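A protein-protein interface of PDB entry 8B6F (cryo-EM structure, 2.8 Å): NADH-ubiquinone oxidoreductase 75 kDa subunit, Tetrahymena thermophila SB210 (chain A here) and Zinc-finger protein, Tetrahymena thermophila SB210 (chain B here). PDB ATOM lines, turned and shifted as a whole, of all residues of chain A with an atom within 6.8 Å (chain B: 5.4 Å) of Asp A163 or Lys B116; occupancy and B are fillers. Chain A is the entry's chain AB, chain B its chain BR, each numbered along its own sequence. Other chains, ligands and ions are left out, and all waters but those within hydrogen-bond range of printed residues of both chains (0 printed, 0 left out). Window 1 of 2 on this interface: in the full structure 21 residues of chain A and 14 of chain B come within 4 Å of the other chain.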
ATOM      1  N   ASP A 128      29.300 -24.697 -16.527  1.00  0.00           N
ATOM      2  CA  ASP A 128      29.596 -23.267 -16.484  1.00  0.00           C
ATOM      3  C   ASP A 128      30.866 -22.939 -15.705  1.00  0.00           C
ATOM      4  O   ASP A 128      31.035 -21.799 -15.266  1.00  0.00           O
ATOM      5  CB  ASP A 128      28.417 -22.511 -15.872  1.00  0.00           C
ATOM      6  CG  ASP A 128      27.167 -22.599 -16.717  1.00  0.00           C
ATOM      7  OD1 ASP A 128      27.238 -23.172 -17.822  1.00  0.00           O
ATOM      8  OD2 ASP A 128      26.112 -22.104 -16.271  1.00  0.00           O
ATOM      9  N   ILE A 131      32.815 -19.955 -17.201  1.00  0.00           N
ATOM     10  CA  ILE A 131      32.127 -18.670 -17.107  1.00  0.00           C
ATOM     11  C   ILE A 131      31.696 -18.339 -15.684  1.00  0.00           C
ATOM     12  O   ILE A 131      31.306 -17.191 -15.424  1.00  0.00           O
ATOM     13  CB  ILE A 131      30.892 -18.595 -18.033  1.00  0.00           C
ATOM     14  CG1 ILE A 131      29.932 -19.754 -17.759  1.00  0.00           C
ATOM     15  CG2 ILE A 131      31.324 -18.605 -19.482  1.00  0.00           C
ATOM     16  CD1 ILE A 131      28.636 -19.672 -18.540  1.00  0.00           C
ATOM     17  N   VAL A 161      16.824 -23.364 -15.202  1.00  0.00           N
ATOM     18  CA  VAL A 161      16.090 -22.461 -14.325  1.00  0.00           C
ATOM     19  C   VAL A 161      16.332 -21.031 -14.781  1.00  0.00           C
ATOM     20  O   VAL A 161      17.465 -20.655 -15.103  1.00  0.00           O
ATOM     21  CB  VAL A 161      16.507 -22.635 -12.849  1.00  0.00           C
ATOM     22  CG1 VAL A 161      15.694 -21.712 -11.951  1.00  0.00           C
ATOM     23  CG2 VAL A 161      16.346 -24.082 -12.416  1.00  0.00           C
ATOM     24  N   GLU A 162      15.267 -20.240 -14.815  1.00  0.00           N
ATOM     25  CA  GLU A 162      15.387 -18.836 -15.177  1.00  0.00           C
ATOM     26  C   GLU A 162      16.168 -18.074 -14.112  1.00  0.00           C
ATOM     27  O   GLU A 162      16.134 -18.406 -12.925  1.00  0.00           O
ATOM     28  CB  GLU A 162      14.004 -18.210 -15.343  1.00  0.00           C
ATOM     29  CG  GLU A 162      14.037 -16.746 -15.744  1.00  0.00           C
ATOM     30  CD  GLU A 162      12.656 -16.140 -15.830  1.00  0.00           C
ATOM     31  OE1 GLU A 162      11.668 -16.901 -15.769  1.00  0.00           O
ATOM     32  OE2 GLU A 162      12.557 -14.902 -15.956  1.00  0.00           O
ATOM     33  N   ASP A 163      16.881 -17.041 -14.553  1.00  0.00           N
ATOM     34  CA  ASP A 163      17.644 -16.206 -13.643  1.00  0.00           C
ATOM     35  C   ASP A 163      16.728 -15.222 -12.921  1.00  0.00           C
ATOM     36  O   ASP A 163      15.587 -14.980 -13.323  1.00  0.00           O
ATOM     37  CB  ASP A 163      18.738 -15.446 -14.392  1.00  0.00           C
ATOM     38  CG  ASP A 163      19.794 -16.366 -14.971  1.00  0.00           C
ATOM     39  OD1 ASP A 163      19.960 -17.486 -14.444  1.00  0.00           O
ATOM     40  OD2 ASP A 163      20.461 -15.969 -15.949  1.00  0.00           O
ATOM     41  N   LYS A 164      17.249 -14.650 -11.840  1.00  0.00           N
ATOM     42  CA  LYS A 164      16.503 -13.731 -10.996  1.00  0.00           C
ATOM     43  C   LYS A 164      17.332 -12.480 -10.745  1.00  0.00           C
ATOM     44  O   LYS A 164      18.565 -12.522 -10.751  1.00  0.00           O
ATOM     45  CB  LYS A 164      16.123 -14.386  -9.664  1.00  0.00           C
ATOM     46  CG  LYS A 164      15.289 -15.646  -9.827  1.00  0.00           C
ATOM     47  CD  LYS A 164      15.075 -16.351  -8.499  1.00  0.00           C
ATOM     48  CE  LYS A 164      14.144 -17.542  -8.655  1.00  0.00           C
ATOM     49  NZ  LYS A 164      14.650 -18.534  -9.645  1.00  0.00           N
ATOM     50  N   ASN A 165      16.640 -11.364 -10.528  1.00  0.00           N
ATOM     51  CA  ASN A 165      17.268 -10.067 -10.307  1.00  0.00           C
ATOM     52  C   ASN A 165      17.164  -9.730  -8.824  1.00  0.00           C
ATOM     53  O   ASN A 165      16.072  -9.440  -8.324  1.00  0.00           O
ATOM     54  CB  ASN A 165      16.602  -8.993 -11.165  1.00  0.00           C
ATOM     55  CG  ASN A 165      17.332  -7.668 -11.113  1.00  0.00           C
ATOM     56  OD1 ASN A 165      18.010  -7.356 -10.134  1.00  0.00           O
ATOM     57  ND2 ASN A 165      17.199  -6.879 -12.172  1.00  0.00           N
ATOM     58  N   THR A 172      22.863 -13.587 -10.012  1.00  0.00           N
ATOM     59  CA  THR A 172      22.242 -14.887  -9.814  1.00  0.00           C
ATOM     60  C   THR A 172      22.316 -15.698 -11.099  1.00  0.00           C
ATOM     61  O   THR A 172      21.935 -15.213 -12.169  1.00  0.00           O
ATOM     62  CB  THR A 172      20.782 -14.735  -9.382  1.00  0.00           C
ATOM     63  OG1 THR A 172      19.997 -14.283 -10.490  1.00  0.00           O
ATOM     64  CG2 THR A 172      20.658 -13.723  -8.257  1.00  0.00           C
ATOM     65  N   SER A 173      22.809 -16.931 -10.988  1.00  0.00           N
ATOM     66  CA  SER A 173      22.776 -17.915 -12.071  1.00  0.00           C
ATOM     67  C   SER A 173      22.197 -19.177 -11.445  1.00  0.00           C
ATOM     68  O   SER A 173      22.934 -20.042 -10.965  1.00  0.00           O
ATOM     69  CB  SER A 173      24.160 -18.147 -12.662  1.00  0.00           C
ATOM     70  OG  SER A 173      24.100 -19.053 -13.748  1.00  0.00           O
ATOM     71  N   MET A 174      20.868 -19.283 -11.457  1.00  0.00           N
ATOM     72  CA  MET A 174      20.202 -20.297 -10.655  1.00  0.00           C
ATOM     73  C   MET A 174      20.361 -21.708 -11.196  1.00  0.00           C
ATOM     74  O   MET A 174      20.016 -22.656 -10.483  1.00  0.00           O
ATOM     75  CB  MET A 174      18.711 -19.973 -10.545  1.00  0.00           C
ATOM     76  CG  MET A 174      18.417 -18.581 -10.018  1.00  0.00           C
ATOM     77  SD  MET A 174      19.352 -18.172  -8.528  1.00  0.00           S
ATOM     78  CE  MET A 174      18.887 -19.521  -7.445  1.00  0.00           C
ATOM     79  N   ASN A 175      20.856 -21.892 -12.420  1.00  0.00           N
ATOM     80  CA  ASN A 175      21.093 -23.259 -12.858  1.00  0.00           C
ATOM     81  C   ASN A 175      22.143 -23.947 -11.993  1.00  0.00           C
ATOM     82  O   ASN A 175      22.133 -25.176 -11.869  1.00  0.00           O
ATOM     83  CB  ASN A 175      21.541 -23.256 -14.321  1.00  0.00           C
ATOM     84  CG  ASN A 175      20.400 -22.993 -15.282  1.00  0.00           C
ATOM     85  OD1 ASN A 175      19.334 -22.527 -14.886  1.00  0.00           O
ATOM     86  ND2 ASN A 175      20.633 -23.258 -16.563  1.00  0.00           N
ATOM     87  N   ARG A 176      23.054 -23.179 -11.388  1.00  0.00           N
ATOM     88  CA  ARG A 176      24.106 -23.743 -10.551  1.00  0.00           C
ATOM     89  C   ARG A 176      23.679 -23.970  -9.105  1.00  0.00           C
ATOM     90  O   ARG A 176      24.482 -24.462  -8.308  1.00  0.00           O
ATOM     91  CB  ARG A 176      25.303 -22.794 -10.564  1.00  0.00           C
ATOM     92  CG  ARG A 176      25.784 -22.426 -11.956  1.00  0.00           C
ATOM     93  CD  ARG A 176      26.598 -21.145 -11.920  1.00  0.00           C
ATOM     94  NE  ARG A 176      26.796 -20.597 -13.256  1.00  0.00           N
ATOM     95  CZ  ARG A 176      27.358 -19.423 -13.510  1.00  0.00           C
ATOM     96  NH1 ARG A 176      27.804 -18.645 -12.540  1.00  0.00           N
ATOM     97  NH2 ARG A 176      27.469 -19.018 -14.772  1.00  0.00           N
ATOM     98  N   ILE B 102      19.215 -23.898 -21.764  1.00  0.00           N
ATOM     99  CA  ILE B 102      18.614 -22.600 -21.481  1.00  0.00           C
ATOM    100  C   ILE B 102      17.112 -22.789 -21.332  1.00  0.00           C
ATOM    101  O   ILE B 102      16.473 -23.423 -22.179  1.00  0.00           O
ATOM    102  CB  ILE B 102      18.930 -21.578 -22.589  1.00  0.00           C
ATOM    103  CG1 ILE B 102      20.443 -21.390 -22.716  1.00  0.00           C
ATOM    104  CG2 ILE B 102      18.247 -20.246 -22.303  1.00  0.00           C
ATOM    105  CD1 ILE B 102      20.864 -20.606 -23.936  1.00  0.00           C
ATOM    106  N   ARG B 107       9.177 -16.619 -16.726  1.00  0.00           N
ATOM    107  CA  ARG B 107       8.029 -16.181 -15.941  1.00  0.00           C
ATOM    108  C   ARG B 107       7.200 -15.139 -16.678  1.00  0.00           C
ATOM    109  O   ARG B 107       6.034 -14.928 -16.326  1.00  0.00           O
ATOM    110  CB  ARG B 107       8.490 -15.623 -14.594  1.00  0.00           C
ATOM    111  CG  ARG B 107       9.374 -14.393 -14.698  1.00  0.00           C
ATOM    112  CD  ARG B 107       9.815 -13.921 -13.323  1.00  0.00           C
ATOM    113  NE  ARG B 107      10.644 -14.912 -12.646  1.00  0.00           N
ATOM    114  CZ  ARG B 107      11.963 -14.991 -12.752  1.00  0.00           C
ATOM    115  NH1 ARG B 107      12.650 -14.149 -13.508  1.00  0.00           N
ATOM    116  NH2 ARG B 107      12.612 -15.938 -12.081  1.00  0.00           N
ATOM    117  N   THR B 114      19.641 -15.238 -23.603  1.00  0.00           N
ATOM    118  CA  THR B 114      20.895 -15.297 -24.340  1.00  0.00           C
ATOM    119  C   THR B 114      21.795 -16.375 -23.755  1.00  0.00           C
ATOM    120  O   THR B 114      21.894 -16.522 -22.534  1.00  0.00           O
ATOM    121  CB  THR B 114      21.610 -13.941 -24.303  1.00  0.00           C
ATOM    122  OG1 THR B 114      22.745 -13.970 -25.177  1.00  0.00           O
ATOM    123  CG2 THR B 114      22.072 -13.599 -22.888  1.00  0.00           C
ATOM    124  N   CYS B 115      22.435 -17.140 -24.634  1.00  0.00           N
ATOM    125  CA  CYS B 115      23.410 -18.125 -24.189  1.00  0.00           C
ATOM    126  C   CYS B 115      24.624 -17.415 -23.601  1.00  0.00           C
ATOM    127  O   CYS B 115      25.015 -16.338 -24.056  1.00  0.00           O
ATOM    128  CB  CYS B 115      23.816 -19.035 -25.349  1.00  0.00           C
ATOM    129  SG  CYS B 115      25.172 -20.168 -24.985  1.00  0.00           S
ATOM    130  N   LYS B 116      25.212 -18.013 -22.565  1.00  0.00           N
ATOM    131  CA  LYS B 116      26.336 -17.376 -21.891  1.00  0.00           C
ATOM    132  C   LYS B 116      27.632 -17.518 -22.682  1.00  0.00           C
ATOM    133  O   LYS B 116      28.450 -16.593 -22.705  1.00  0.00           O
ATOM    134  CB  LYS B 116      26.497 -17.958 -20.488  1.00  0.00           C
ATOM    135  CG  LYS B 116      25.277 -17.740 -19.601  1.00  0.00           C
ATOM    136  CD  LYS B 116      25.526 -18.221 -18.182  1.00  0.00           C
ATOM    137  CE  LYS B 116      24.300 -18.028 -17.305  1.00  0.00           C
ATOM    138  NZ  LYS B 116      23.883 -16.601 -17.220  1.00  0.00           N
ATOM    139  N   TYR B 117      27.843 -18.664 -23.331  1.00  0.00           N
ATOM    140  CA  TYR B 117      29.071 -18.862 -24.096  1.00  0.00           C
ATOM    141  C   TYR B 117      29.052 -18.074 -25.400  1.00  0.00           C
ATOM    142  O   TYR B 117      30.067 -17.486 -25.790  1.00  0.00           O
ATOM    143  CB  TYR B 117      29.273 -20.349 -24.373  1.00  0.00           C
ATOM    144  CG  TYR B 117      29.703 -21.139 -23.161  1.00  0.00           C
ATOM    145  CD1 TYR B 117      31.045 -21.264 -22.833  1.00  0.00           C
ATOM    146  CD2 TYR B 117      28.768 -21.761 -22.348  1.00  0.00           C
ATOM    147  CE1 TYR B 117      31.443 -21.985 -21.730  1.00  0.00           C
ATOM    148  CE2 TYR B 117      29.157 -22.484 -21.242  1.00  0.00           C
ATOM    149  CZ  TYR B 117      30.497 -22.592 -20.938  1.00  0.00           C
ATOM    150  OH  TYR B 117      30.893 -23.312 -19.838  1.00  0.00           O
ATOM    151  N   CYS B 118      27.917 -18.057 -26.092  1.00  0.00           N
ATOM    152  CA  CYS B 118      27.754 -17.299 -27.323  1.00  0.00           C
ATOM    153  C   CYS B 118      26.519 -16.421 -27.188  1.00  0.00           C
ATOM    154  O   CYS B 118      25.603 -16.727 -26.423  1.00  0.00           O
ATOM    155  CB  CYS B 118      27.638 -18.205 -28.560  1.00  0.00           C
ATOM    156  SG  CYS B 118      26.364 -19.476 -28.474  1.00  0.00           S
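Of the printed residues of chain B, Ile A131 touches Lys B116 (3.4 Å) and Tyr B117 (3.9 Å). Of the printed residues of chain B, Glu A162 touches Arg B107. Asp A163 touches two residues of chain B. Printed residues of chain B within 4 Å of Lys A164: Arg B107 (3.5 Å). Thr A172 touches none of the printed residues of chain B. Printed residues of chain B within 4 Å of Ser A173: Lys B116. Of the printed residues of chain A, Arg B107 touches Glu A162, Asp A163 and Lys A164. Thr B114 touches none of the printed residues of chain A. Of the printed residues of chain A, Lys B116 touches Ile A131 (3.4 Å), Asp A163 (3.7 Å) and Ser A173 (3.7 Å). The nearest printed residue of chain A that does not touch Lys B116 is Arg A176 (4.005 Å).
Of the 12 printed residues of chain A, 6 touch a printed residue of chain B. Printed residues of chain A that touch a printed residue of chain B: Asp A128, Ile A131, Glu A162, Asp A163, Lys A164 and Ser A173. Hydrophobic or aromatic side chains of chain A within 4 Å of the printed part of chain B: Ile A131. Printed residues of chain B that touch a printed residue of chain A: Arg B107, Lys B116 and Tyr B117.
Among the printed residues, merely in contact across the chains: Ile A131 with Lys B116 (3.4 Å), Lys A164 with Arg B107 (3.5 Å), Asp A128 with Tyr B117 (3.6 Å), Ser A173 with Lys B116 (3.7 Å) and Ile A131 with Tyr B117 (3.9 Å).
O of Asp A163 is in hydrogen-bond range of NH1 of Arg B107, at 3.1 Å. The side-chain carboxylate of Asp A163 is in salt-bridge range of the side-chain amino group of Lys B116 (3.7 Å). The side-chain carboxylate (OE2) of Glu A162 lies within salt-bridge range of the guanidinium group (NH1) of Arg B107 (2.6 Å).
NE of Arg A176 is in salt-bridge range of OD2 of Asp A128, 3.4 Å away. The backbone NH (N) of Lys A164 lies within hydrogen-bond range of the side-chain hydroxyl (OG1) of Thr A172 (3.1 Å). The side-chain hydroxyl (OG) of Ser A173 sits at hydrogen-bond distance from the guanidinium group (NE) of Arg A176, 3.1 Å away. The backbone NH of Tyr B117 lies close to the side-chain sulfur of Cys B115 (3.5 Å).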
